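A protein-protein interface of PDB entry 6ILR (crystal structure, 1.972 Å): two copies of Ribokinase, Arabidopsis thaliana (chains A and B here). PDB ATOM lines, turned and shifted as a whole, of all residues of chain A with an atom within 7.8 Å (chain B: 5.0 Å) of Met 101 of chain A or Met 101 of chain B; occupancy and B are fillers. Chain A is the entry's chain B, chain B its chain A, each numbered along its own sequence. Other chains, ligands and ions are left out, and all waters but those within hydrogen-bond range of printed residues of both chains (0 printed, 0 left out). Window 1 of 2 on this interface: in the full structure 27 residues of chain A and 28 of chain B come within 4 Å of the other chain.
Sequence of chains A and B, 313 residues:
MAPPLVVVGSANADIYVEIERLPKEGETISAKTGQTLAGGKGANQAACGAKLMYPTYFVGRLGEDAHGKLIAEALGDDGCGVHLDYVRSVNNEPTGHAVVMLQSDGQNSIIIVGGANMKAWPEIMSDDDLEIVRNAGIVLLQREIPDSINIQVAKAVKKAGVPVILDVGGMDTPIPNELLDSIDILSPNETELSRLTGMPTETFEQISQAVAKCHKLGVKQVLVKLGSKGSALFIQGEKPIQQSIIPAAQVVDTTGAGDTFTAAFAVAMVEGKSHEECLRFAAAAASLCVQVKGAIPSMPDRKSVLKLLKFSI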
ATOM      1  N   ILE A  15       7.662  -2.991   9.264  1.00  0.00           N
ATOM      2  CA  ILE A  15       8.176  -2.788   7.914  1.00  0.00           C
ATOM      3  C   ILE A  15       7.615  -1.500   7.316  1.00  0.00           C
ATOM      4  O   ILE A  15       6.499  -1.485   6.795  1.00  0.00           O
ATOM      5  CB  ILE A  15       7.811  -3.953   6.986  1.00  0.00           C
ATOM      6  CG1 ILE A  15       8.076  -5.306   7.653  1.00  0.00           C
ATOM      7  CG2 ILE A  15       8.555  -3.825   5.661  1.00  0.00           C
ATOM      8  CD1 ILE A  15       9.521  -5.607   7.834  1.00  0.00           C
ATOM      9  N   TYR A  16       8.385  -0.421   7.406  1.00  0.00           N
ATOM     10  CA  TYR A  16       7.962   0.872   6.875  1.00  0.00           C
ATOM     11  C   TYR A  16       8.387   1.033   5.431  1.00  0.00           C
ATOM     12  O   TYR A  16       9.547   0.804   5.108  1.00  0.00           O
ATOM     13  CB  TYR A  16       8.554   2.016   7.695  1.00  0.00           C
ATOM     14  CG  TYR A  16       8.067   2.063   9.115  1.00  0.00           C
ATOM     15  CD1 TYR A  16       6.842   2.634   9.428  1.00  0.00           C
ATOM     16  CD2 TYR A  16       8.834   1.544  10.148  1.00  0.00           C
ATOM     17  CE1 TYR A  16       6.387   2.680  10.732  1.00  0.00           C
ATOM     18  CE2 TYR A  16       8.392   1.589  11.458  1.00  0.00           C
ATOM     19  CZ  TYR A  16       7.166   2.156  11.744  1.00  0.00           C
ATOM     20  OH  TYR A  16       6.721   2.197  13.048  1.00  0.00           O
ATOM     21  N   VAL A  17       7.456   1.436   4.569  1.00  0.00           N
ATOM     22  CA  VAL A  17       7.793   1.767   3.188  1.00  0.00           C
ATOM     23  C   VAL A  17       7.204   3.126   2.791  1.00  0.00           C
ATOM     24  O   VAL A  17       6.039   3.417   3.065  1.00  0.00           O
ATOM     25  CB  VAL A  17       7.307   0.682   2.207  1.00  0.00           C
ATOM     26  CG1 VAL A  17       8.108  -0.602   2.397  1.00  0.00           C
ATOM     27  CG2 VAL A  17       5.819   0.415   2.376  1.00  0.00           C
ATOM     28  N   GLU A  18       8.028   3.962   2.167  1.00  0.00           N
ATOM     29  CA  GLU A  18       7.587   5.269   1.685  1.00  0.00           C
ATOM     30  C   GLU A  18       7.095   5.171   0.250  1.00  0.00           C
ATOM     31  O   GLU A  18       7.880   4.960  -0.676  1.00  0.00           O
ATOM     32  CB  GLU A  18       8.717   6.297   1.775  1.00  0.00           C
ATOM     33  CG  GLU A  18       8.923   6.883   3.158  1.00  0.00           C
ATOM     34  CD  GLU A  18      10.014   7.939   3.193  1.00  0.00           C
ATOM     35  OE1 GLU A  18      10.144   8.700   2.206  1.00  0.00           O
ATOM     36  OE2 GLU A  18      10.742   8.003   4.208  1.00  0.00           O
ATOM     37  N   ILE A  19       5.790   5.323   0.066  1.00  0.00           N
ATOM     38  CA  ILE A  19       5.207   5.295  -1.265  1.00  0.00           C
ATOM     39  C   ILE A  19       4.545   6.630  -1.589  1.00  0.00           C
ATOM     40  O   ILE A  19       4.245   7.418  -0.686  1.00  0.00           O
ATOM     41  CB  ILE A  19       4.180   4.162  -1.397  1.00  0.00           C
ATOM     42  CG1 ILE A  19       3.059   4.337  -0.369  1.00  0.00           C
ATOM     43  CG2 ILE A  19       4.859   2.813  -1.214  1.00  0.00           C
ATOM     44  CD1 ILE A  19       2.022   3.232  -0.403  1.00  0.00           C
ATOM     45  N   ARG A  21       1.604   6.874  -3.612  1.00  0.00           N
ATOM     46  CA  ARG A  21       0.199   6.542  -3.432  1.00  0.00           C
ATOM     47  C   ARG A  21       0.062   5.058  -3.136  1.00  0.00           C
ATOM     48  O   ARG A  21       0.952   4.272  -3.458  1.00  0.00           O
ATOM     49  CB  ARG A  21      -0.606   6.895  -4.679  1.00  0.00           C
ATOM     50  CG  ARG A  21      -0.133   6.153  -5.918  1.00  0.00           C
ATOM     51  CD  ARG A  21      -1.146   6.231  -7.049  1.00  0.00           C
ATOM     52  NE  ARG A  21      -0.637   5.611  -8.269  1.00  0.00           N
ATOM     53  CZ  ARG A  21      -0.715   4.311  -8.539  1.00  0.00           C
ATOM     54  NH1 ARG A  21      -1.286   3.484  -7.673  1.00  0.00           N
ATOM     55  NH2 ARG A  21      -0.221   3.838  -9.674  1.00  0.00           N
ATOM     56  N   LEU A  22      -1.054   4.674  -2.528  1.00  0.00           N
ATOM     57  CA  LEU A  22      -1.347   3.264  -2.330  1.00  0.00           C
ATOM     58  C   LEU A  22      -1.566   2.589  -3.682  1.00  0.00           C
ATOM     59  O   LEU A  22      -2.286   3.112  -4.530  1.00  0.00           O
ATOM     60  CB  LEU A  22      -2.574   3.084  -1.434  1.00  0.00           C
ATOM     61  CG  LEU A  22      -2.586   3.909  -0.146  1.00  0.00           C
ATOM     62  CD1 LEU A  22      -3.998   4.062   0.396  1.00  0.00           C
ATOM     63  CD2 LEU A  22      -1.679   3.271   0.895  1.00  0.00           C
ATOM     64  N   PRO A  23      -0.938   1.424  -3.888  1.00  0.00           N
ATOM     65  CA  PRO A  23      -1.050   0.707  -5.161  1.00  0.00           C
ATOM     66  C   PRO A  23      -2.470   0.236  -5.430  1.00  0.00           C
ATOM     67  O   PRO A  23      -3.191  -0.123  -4.499  1.00  0.00           O
ATOM     68  CB  PRO A  23      -0.110  -0.485  -4.974  1.00  0.00           C
ATOM     69  CG  PRO A  23      -0.088  -0.704  -3.501  1.00  0.00           C
ATOM     70  CD  PRO A  23      -0.157   0.665  -2.896  1.00  0.00           C
ATOM     71  N   GLU A  25      -5.293  -2.409  -7.173  1.00  0.00           N
ATOM     72  CA  GLU A  25      -5.395  -3.860  -7.271  1.00  0.00           C
ATOM     73  C   GLU A  25      -4.687  -4.374  -8.522  1.00  0.00           C
ATOM     74  O   GLU A  25      -4.846  -3.822  -9.608  1.00  0.00           O
ATOM     75  CB  GLU A  25      -6.864  -4.295  -7.277  1.00  0.00           C
ATOM     76  N   GLY A  26      -3.887  -5.421  -8.356  1.00  0.00           N
ATOM     77  CA  GLY A  26      -3.169  -6.015  -9.468  1.00  0.00           C
ATOM     78  C   GLY A  26      -1.981  -5.195  -9.939  1.00  0.00           C
ATOM     79  O   GLY A  26      -1.244  -5.626 -10.829  1.00  0.00           O
ATOM     80  N   GLU A  27      -1.784  -4.023  -9.340  1.00  0.00           N
ATOM     81  CA  GLU A  27      -0.736  -3.105  -9.785  1.00  0.00           C
ATOM     82  C   GLU A  27       0.537  -3.169  -8.942  1.00  0.00           C
ATOM     83  O   GLU A  27       0.485  -3.180  -7.709  1.00  0.00           O
ATOM     84  CB  GLU A  27      -1.251  -1.665  -9.787  1.00  0.00           C
ATOM     85  CG  GLU A  27      -0.267  -0.681 -10.405  1.00  0.00           C
ATOM     86  CD  GLU A  27      -0.485   0.743  -9.943  1.00  0.00           C
ATOM     87  OE1 GLU A  27      -1.328   0.959  -9.045  1.00  0.00           O
ATOM     88  OE2 GLU A  27       0.194   1.646 -10.475  1.00  0.00           O
ATOM     89  N   ILE A  29       3.938  -1.229  -7.842  1.00  0.00           N
ATOM     90  CA  ILE A  29       4.553   0.095  -7.778  1.00  0.00           C
ATOM     91  C   ILE A  29       5.911   0.065  -7.088  1.00  0.00           C
ATOM     92  O   ILE A  29       6.295  -0.948  -6.499  1.00  0.00           O
ATOM     93  CB  ILE A  29       3.662   1.106  -7.041  1.00  0.00           C
ATOM     94  CG1 ILE A  29       3.648   0.809  -5.539  1.00  0.00           C
ATOM     95  CG2 ILE A  29       2.258   1.108  -7.625  1.00  0.00           C
ATOM     96  CD1 ILE A  29       2.931   1.855  -4.720  1.00  0.00           C
ATOM     97  N   ALA A  98       4.320  -5.900  10.834  1.00  0.00           N
ATOM     98  CA  ALA A  98       3.383  -4.917  10.329  1.00  0.00           C
ATOM     99  C   ALA A  98       3.980  -4.184   9.139  1.00  0.00           C
ATOM    100  O   ALA A  98       5.057  -3.597   9.239  1.00  0.00           O
ATOM    101  CB  ALA A  98       3.003  -3.927  11.431  1.00  0.00           C
ATOM    102  N   VAL A  99       3.280  -4.227   8.015  1.00  0.00           N
ATOM    103  CA  VAL A  99       3.654  -3.414   6.867  1.00  0.00           C
ATOM    104  C   VAL A  99       2.991  -2.040   6.986  1.00  0.00           C
ATOM    105  O   VAL A  99       1.777  -1.902   6.832  1.00  0.00           O
ATOM    106  CB  VAL A  99       3.254  -4.082   5.549  1.00  0.00           C
ATOM    107  CG1 VAL A  99       3.729  -3.248   4.368  1.00  0.00           C
ATOM    108  CG2 VAL A  99       3.822  -5.498   5.486  1.00  0.00           C
ATOM    109  N   VAL A 100       3.797  -1.032   7.290  1.00  0.00           N
ATOM    110  CA  VAL A 100       3.310   0.330   7.440  1.00  0.00           C
ATOM    111  C   VAL A 100       3.673   1.162   6.214  1.00  0.00           C
ATOM    112  O   VAL A 100       4.850   1.413   5.952  1.00  0.00           O
ATOM    113  CB  VAL A 100       3.891   0.999   8.697  1.00  0.00           C
ATOM    114  CG1 VAL A 100       3.349   2.411   8.841  1.00  0.00           C
ATOM    115  CG2 VAL A 100       3.583   0.168   9.936  1.00  0.00           C
ATOM    116  N   MET A 101       2.661   1.589   5.466  1.00  0.00           N
ATOM    117  CA  MET A 101       2.886   2.335   4.233  1.00  0.00           C
ATOM    118  C   MET A 101       2.666   3.831   4.432  1.00  0.00           C
ATOM    119  O   MET A 101       1.539   4.286   4.608  1.00  0.00           O
ATOM    120  CB  MET A 101       1.977   1.801   3.127  1.00  0.00           C
ATOM    121  CG  MET A 101       1.712   0.322   3.279  1.00  0.00           C
ATOM    122  SD  MET A 101       0.890  -0.456   1.891  1.00  0.00           S
ATOM    123  CE  MET A 101       0.041  -1.788   2.735  1.00  0.00           C
ATOM    124  N   LEU A 102       3.759   4.586   4.414  1.00  0.00           N
ATOM    125  CA  LEU A 102       3.706   6.034   4.535  1.00  0.00           C
ATOM    126  C   LEU A 102       3.497   6.678   3.162  1.00  0.00           C
ATOM    127  O   LEU A 102       4.438   6.788   2.374  1.00  0.00           O
ATOM    128  CB  LEU A 102       4.993   6.560   5.170  1.00  0.00           C
ATOM    129  CG  LEU A 102       5.511   5.846   6.421  1.00  0.00           C
ATOM    130  CD1 LEU A 102       6.915   6.329   6.764  1.00  0.00           C
ATOM    131  CD2 LEU A 102       4.573   6.068   7.595  1.00  0.00           C
ATOM    132  N   GLN A 103       2.266   7.092   2.868  1.00  0.00           N
ATOM    133  CA  GLN A 103       1.993   7.801   1.618  1.00  0.00           C
ATOM    134  C   GLN A 103       2.520   9.229   1.688  1.00  0.00           C
ATOM    135  O   GLN A 103       2.857   9.728   2.762  1.00  0.00           O
ATOM    136  CB  GLN A 103       0.497   7.808   1.288  1.00  0.00           C
ATOM    137  CG  GLN A 103      -0.433   7.997   2.480  1.00  0.00           C
ATOM    138  CD  GLN A 103      -0.871   6.679   3.087  1.00  0.00           C
ATOM    139  OE1 GLN A 103      -0.501   5.613   2.599  1.00  0.00           O
ATOM    140  NE2 GLN A 103      -1.672   6.743   4.143  1.00  0.00           N
ATOM    141  N   SER A 104       2.597   9.877   0.533  1.00  0.00           N
ATOM    142  CA  SER A 104       3.193  11.206   0.439  1.00  0.00           C
ATOM    143  C   SER A 104       2.281  12.321   0.956  1.00  0.00           C
ATOM    144  O   SER A 104       2.759  13.416   1.258  1.00  0.00           O
ATOM    145  CB  SER A 104       3.596  11.494  -1.008  1.00  0.00           C
ATOM    146  OG  SER A 104       2.656  10.944  -1.916  1.00  0.00           O
ATOM    147  N   ASP A 105       0.980  12.051   1.067  1.00  0.00           N
ATOM    148  CA  ASP A 105       0.043  13.075   1.528  1.00  0.00           C
ATOM    149  C   ASP A 105       0.207  13.350   3.026  1.00  0.00           C
ATOM    150  O   ASP A 105       0.028  14.479   3.482  1.00  0.00           O
ATOM    151  CB  ASP A 105      -1.410  12.686   1.190  1.00  0.00           C
ATOM    152  CG  ASP A 105      -1.891  11.430   1.912  1.00  0.00           C
ATOM    153  OD1 ASP A 105      -1.234  10.960   2.865  1.00  0.00           O
ATOM    154  OD2 ASP A 105      -2.953  10.904   1.511  1.00  0.00           O
ATOM    155  N   GLY A 106       0.554  12.314   3.782  1.00  0.00           N
ATOM    156  CA  GLY A 106       0.818  12.468   5.201  1.00  0.00           C
ATOM    157  C   GLY A 106       0.140  11.428   6.073  1.00  0.00           C
ATOM    158  O   GLY A 106       0.508  11.256   7.234  1.00  0.00           O
ATOM    159  N   GLN A 107      -0.852  10.735   5.520  1.00  0.00           N
ATOM    160  CA  GLN A 107      -1.569   9.703   6.260  1.00  0.00           C
ATOM    161  C   GLN A 107      -0.726   8.436   6.397  1.00  0.00           C
ATOM    162  O   GLN A 107       0.402   8.369   5.909  1.00  0.00           O
ATOM    163  CB  GLN A 107      -2.903   9.389   5.575  1.00  0.00           C
ATOM    164  N   ASN A 108      -1.271   7.436   7.080  1.00  0.00           N
ATOM    165  CA  ASN A 108      -0.600   6.150   7.220  1.00  0.00           C
ATOM    166  C   ASN A 108      -1.541   5.027   6.799  1.00  0.00           C
ATOM    167  O   ASN A 108      -2.750   5.222   6.685  1.00  0.00           O
ATOM    168  CB  ASN A 108      -0.112   5.934   8.659  1.00  0.00           C
ATOM    169  CG  ASN A 108      -1.254   5.769   9.647  1.00  0.00           C
ATOM    170  OD1 ASN A 108      -1.905   6.740  10.037  1.00  0.00           O
ATOM    171  ND2 ASN A 108      -1.498   4.533  10.059  1.00  0.00           N
ATOM    172  N   SER A 109      -0.980   3.853   6.550  1.00  0.00           N
ATOM    173  CA  SER A 109      -1.780   2.682   6.219  1.00  0.00           C
ATOM    174  C   SER A 109      -1.050   1.418   6.660  1.00  0.00           C
ATOM    175  O   SER A 109       0.132   1.242   6.365  1.00  0.00           O
ATOM    176  CB  SER A 109      -2.078   2.642   4.724  1.00  0.00           C
ATOM    177  OG  SER A 109      -2.848   3.765   4.340  1.00  0.00           O
ATOM    178  N   ILE A 110      -1.749   0.540   7.372  1.00  0.00           N
ATOM    179  CA  ILE A 110      -1.087  -0.567   8.052  1.00  0.00           C
ATOM    180  C   ILE A 110      -1.741  -1.921   7.791  1.00  0.00           C
ATOM    181  O   ILE A 110      -2.961  -2.055   7.846  1.00  0.00           O
ATOM    182  CB  ILE A 110      -1.035  -0.306   9.583  1.00  0.00           C
ATOM    183  CG1 ILE A 110      -0.299   1.007   9.875  1.00  0.00           C
ATOM    184  CG2 ILE A 110      -0.379  -1.465  10.321  1.00  0.00           C
ATOM    185  CD1 ILE A 110      -0.042   1.274  11.342  1.00  0.00           C
ATOM    186  N   ILE A 111      -0.913  -2.917   7.482  1.00  0.00           N
ATOM    187  CA  ILE A 111      -1.338  -4.314   7.465  1.00  0.00           C
ATOM    188  C   ILE A 111      -0.621  -5.062   8.583  1.00  0.00           C
ATOM    189  O   ILE A 111       0.603  -4.994   8.694  1.00  0.00           O
ATOM    190  CB  ILE A 111      -1.037  -5.005   6.126  1.00  0.00           C
ATOM    191  CG1 ILE A 111      -1.748  -4.294   4.974  1.00  0.00           C
ATOM    192  CG2 ILE A 111      -1.453  -6.469   6.179  1.00  0.00           C
ATOM    193  CD1 ILE A 111      -1.582  -4.998   3.639  1.00  0.00           C
ATOM    194  N   VAL B  17       2.015 -11.349   2.261  1.00  0.00           N
ATOM    195  CA  VAL B  17       0.890 -11.249   3.185  1.00  0.00           C
ATOM    196  C   VAL B  17      -0.420 -11.634   2.490  1.00  0.00           C
ATOM    197  O   VAL B  17      -0.720 -11.152   1.397  1.00  0.00           O
ATOM    198  CB  VAL B  17       0.757  -9.823   3.781  1.00  0.00           C
ATOM    199  CG1 VAL B  17       1.817  -9.581   4.848  1.00  0.00           C
ATOM    200  CG2 VAL B  17       0.836  -8.766   2.691  1.00  0.00           C
ATOM    201  N   ILE B  19      -4.261 -11.194   2.526  1.00  0.00           N
ATOM    202  CA  ILE B  19      -5.248 -10.276   3.087  1.00  0.00           C
ATOM    203  C   ILE B  19      -6.606 -10.387   2.401  1.00  0.00           C
ATOM    204  O   ILE B  19      -6.707 -10.854   1.267  1.00  0.00           O
ATOM    205  CB  ILE B  19      -4.769  -8.818   2.990  1.00  0.00           C
ATOM    206  CG1 ILE B  19      -4.483  -8.452   1.535  1.00  0.00           C
ATOM    207  CG2 ILE B  19      -3.531  -8.606   3.842  1.00  0.00           C
ATOM    208  CD1 ILE B  19      -4.205  -6.985   1.323  1.00  0.00           C
ATOM    209  N   LEU B  22      -7.542  -4.540   0.343  1.00  0.00           N
ATOM    210  CA  LEU B  22      -6.518  -3.526   0.556  1.00  0.00           C
ATOM    211  C   LEU B  22      -6.986  -2.483   1.570  1.00  0.00           C
ATOM    212  O   LEU B  22      -8.167  -2.147   1.615  1.00  0.00           O
ATOM    213  CB  LEU B  22      -6.158  -2.853  -0.771  1.00  0.00           C
ATOM    214  CG  LEU B  22      -5.156  -3.604  -1.650  1.00  0.00           C
ATOM    215  CD1 LEU B  22      -5.017  -2.949  -3.018  1.00  0.00           C
ATOM    216  CD2 LEU B  22      -3.811  -3.696  -0.948  1.00  0.00           C
ATOM    217  N   PRO B  23      -6.061  -1.972   2.394  1.00  0.00           N
ATOM    218  CA  PRO B  23      -6.403  -0.913   3.352  1.00  0.00           C
ATOM    219  C   PRO B  23      -6.580   0.446   2.672  1.00  0.00           C
ATOM    220  O   PRO B  23      -6.173   0.611   1.521  1.00  0.00           O
ATOM    221  CB  PRO B  23      -5.199  -0.898   4.299  1.00  0.00           C
ATOM    222  CG  PRO B  23      -4.065  -1.356   3.446  1.00  0.00           C
ATOM    223  CD  PRO B  23      -4.649  -2.380   2.504  1.00  0.00           C
ATOM    224  N   VAL B  99       6.927  -6.068  -1.005  1.00  0.00           N
ATOM    225  CA  VAL B  99       5.736  -6.414  -0.244  1.00  0.00           C
ATOM    226  C   VAL B  99       4.673  -6.968  -1.186  1.00  0.00           C
ATOM    227  O   VAL B  99       4.087  -6.235  -1.983  1.00  0.00           O
ATOM    228  CB  VAL B  99       5.181  -5.203   0.524  1.00  0.00           C
ATOM    229  CG1 VAL B  99       3.862  -5.564   1.207  1.00  0.00           C
ATOM    230  CG2 VAL B  99       6.203  -4.711   1.546  1.00  0.00           C
ATOM    231  N   VAL B 100       4.442  -8.273  -1.102  1.00  0.00           N
ATOM    232  CA  VAL B 100       3.469  -8.927  -1.965  1.00  0.00           C
ATOM    233  C   VAL B 100       2.162  -9.188  -1.222  1.00  0.00           C
ATOM    234  O   VAL B 100       2.079 -10.079  -0.371  1.00  0.00           O
ATOM    235  CB  VAL B 100       4.015 -10.253  -2.522  1.00  0.00           C
ATOM    236  CG1 VAL B 100       3.014 -10.874  -3.475  1.00  0.00           C
ATOM    237  CG2 VAL B 100       5.345 -10.022  -3.225  1.00  0.00           C
ATOM    238  N   MET B 101       1.140  -8.404  -1.551  1.00  0.00           N
ATOM    239  CA  MET B 101      -0.167  -8.538  -0.916  1.00  0.00           C
ATOM    240  C   MET B 101      -1.124  -9.349  -1.784  1.00  0.00           C
ATOM    241  O   MET B 101      -1.689  -8.837  -2.752  1.00  0.00           O
ATOM    242  CB  MET B 101      -0.762  -7.162  -0.629  1.00  0.00           C
ATOM    243  CG  MET B 101       0.265  -6.058  -0.583  1.00  0.00           C
ATOM    244  SD  MET B 101      -0.413  -4.513   0.011  1.00  0.00           S
ATOM    245  CE  MET B 101       0.926  -3.389  -0.370  1.00  0.00           C
ATOM    246  N   LEU B 102      -1.289 -10.619  -1.429  1.00  0.00           N
ATOM    247  CA  LEU B 102      -2.230 -11.503  -2.103  1.00  0.00           C
ATOM    248  C   LEU B 102      -3.638 -11.297  -1.546  1.00  0.00           C
ATOM    249  O   LEU B 102      -3.897 -11.593  -0.378  1.00  0.00           O
ATOM    250  CB  LEU B 102      -1.805 -12.966  -1.938  1.00  0.00           C
ATOM    251  CG  LEU B 102      -0.309 -13.260  -2.092  1.00  0.00           C
ATOM    252  CD1 LEU B 102       0.041 -14.635  -1.535  1.00  0.00           C
ATOM    253  CD2 LEU B 102       0.121 -13.151  -3.544  1.00  0.00           C
ATOM    254  N   GLN B 103      -4.541 -10.787  -2.377  1.00  0.00           N
ATOM    255  CA  GLN B 103      -5.915 -10.529  -1.952  1.00  0.00           C
ATOM    256  C   GLN B 103      -6.760 -11.799  -2.024  1.00  0.00           C
ATOM    257  O   GLN B 103      -6.303 -12.827  -2.529  1.00  0.00           O
ATOM    258  CB  GLN B 103      -6.543  -9.424  -2.802  1.00  0.00           C
ATOM    259  N   GLN B 107      -5.737 -11.595  -7.163  1.00  0.00           N
ATOM    260  CA  GLN B 107      -5.110 -10.320  -7.505  1.00  0.00           C
ATOM    261  C   GLN B 107      -3.997  -9.947  -6.529  1.00  0.00           C
ATOM    262  O   GLN B 107      -4.187  -9.967  -5.312  1.00  0.00           O
ATOM    263  CB  GLN B 107      -6.149  -9.198  -7.543  1.00  0.00           C
ATOM    264  CG  GLN B 107      -7.030  -9.191  -8.777  1.00  0.00           C
ATOM    265  CD  GLN B 107      -7.187  -7.798  -9.356  1.00  0.00           C
ATOM    266  OE1 GLN B 107      -7.902  -6.962  -8.805  1.00  0.00           O
ATOM    267  NE2 GLN B 107      -6.506  -7.538 -10.466  1.00  0.00           N
ATOM    268  N   ASN B 108      -2.839  -9.594  -7.079  1.00  0.00           N
ATOM    269  CA  ASN B 108      -1.667  -9.262  -6.280  1.00  0.00           C
ATOM    270  C   ASN B 108      -1.279  -7.799  -6.424  1.00  0.00           C
ATOM    271  O   ASN B 108      -1.074  -7.316  -7.533  1.00  0.00           O
ATOM    272  CB  ASN B 108      -0.485 -10.145  -6.681  1.00  0.00           C
ATOM    273  CG  ASN B 108      -0.815 -11.624  -6.618  1.00  0.00           C
ATOM    274  OD1 ASN B 108      -1.716 -12.045  -5.888  1.00  0.00           O
ATOM    275  ND2 ASN B 108      -0.083 -12.426  -7.387  1.00  0.00           N
ATOM    276  N   SER B 109      -1.186  -7.097  -5.302  1.00  0.00           N
ATOM    277  CA  SER B 109      -0.628  -5.749  -5.286  1.00  0.00           C
ATOM    278  C   SER B 109       0.779  -5.792  -4.699  1.00  0.00           C
ATOM    279  O   SER B 109       0.992  -6.348  -3.621  1.00  0.00           O
ATOM    280  CB  SER B 109      -1.515  -4.800  -4.480  1.00  0.00           C
ATOM    281  OG  SER B 109      -2.841  -4.799  -4.976  1.00  0.00           O
ATOM    282  N   ILE B 111       4.527  -3.779  -3.756  1.00  0.00           N
ATOM    283  CA  ILE B 111       5.389  -2.619  -3.586  1.00  0.00           C
ATOM    284  C   ILE B 111       6.842  -3.087  -3.645  1.00  0.00           C
ATOM    285  O   ILE B 111       7.212  -4.061  -2.991  1.00  0.00           O
ATOM    286  CB  ILE B 111       5.125  -1.889  -2.267  1.00  0.00           C
ATOM    287  CG1 ILE B 111       3.649  -1.518  -2.144  1.00  0.00           C
ATOM    288  CG2 ILE B 111       5.979  -0.635  -2.172  1.00  0.00           C
ATOM    289  CD1 ILE B 111       3.330  -0.716  -0.888  1.00  0.00           C
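Ile 19 of chain A touches Ile 111 of chain B, and with the chains exchanged Ile 111 of chain A touches Ile 19 of chain B. Pro 23 of chain A touches Leu 22 of chain B, but with the chains exchanged Leu 22 of chain A does not touch Pro 23 of chain B (4.2 Å). Val 99 of chain A touches its own counterpart, Val 99 of chain B. Met 101 of chain A touches its own counterpart, Met 101 of chain B. Of the 15 pairs that touch across the chains among the printed residues, 6 have their exchanged pair printed and touching as well.
The backbone carbonyl oxygen (O) of Asn 108 of chain B sits close to the backbone NH (N) of Gly 26 of chain A, at 3.5 Å.
Of the printed residues of chain B, Glu 25 of chain A touches Gln 107 and Ser 109. Printed residues of chain B within 4 Å of Gly 26 of chain A: Gln 107 (3.8 Å), Asn 108 (3.1 Å) and Ser 109 (3.6 Å). Met 101 of chain A touches just these residues of chain B: Met 101 and Ile 111. Of chain A, only Met 101 (3.6 Å) and Ile 111 (3.8 Å) come within 4 Å of Met 101 of chain B.
Printed residues of chain B that touch a printed residue of chain A: Ile 19, Leu 22, Val 99, Met 101, Gln 107, Asn 108, Ser 109 and Ile 111. Among the printed residues, 15 pairs touch across the chains.
CG2 of Ile 111 of chain B touches CG2 of Ile 19 of chain A, at 3.7 Å. CD1 of Leu 22 of chain B touches O of Pro 23 of chain A, at 3.7 Å. CB of Glu 25 of chain A touches OE1 of Gln 107 of chain B, 3.2 Å away. Ser 109 of chain B touches Glu 25 of chain A (OG to CA, 3.6 Å). Gly 26 of chain A touches Gln 107 of chain B (CA to NE2, 3.8 Å). Gly 26 of chain A touches Ser 109 of chain B (N to OG, 3.6 Å). Glu 27 of chain A touches Ser 109 of chain B. CG1 of Val 99 of chain B touches CG1 of Val 99 of chain A, 3.9 Å away. Met 101 of chain A touches Met 101 of chain B (CE to CE, 3.6 Å). Ile 111 of chain A touches Met 101 of chain B (CD1 to SD, 3.8 Å).
N of Ile 19 of chain B lies within hydrogen-bond range of O of Leu 102 of chain B (3.0 Å). The backbone NH (N) of Met 101 of chain B lies within hydrogen-bond range of the backbone carbonyl oxygen (O) of Ser 109 of chain B (2.9 Å). The backbone NH of Ile 19 of chain A sits at hydrogen-bond distance from the backbone carbonyl oxygen of Leu 102 of chain A, 3.0 Å away. NH1 of Arg 21 of chain A lies within salt-bridge range of OE1 of Glu 27 of chain A (2.9 Å). N of Val 99 of chain A sits at hydrogen-bond distance from O of Ile 111 of chain A. The backbone NH (N) of Met 101 of chain A lies within hydrogen-bond range of the backbone carbonyl oxygen (O) of Ser 109 of chain A (2.7 Å).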
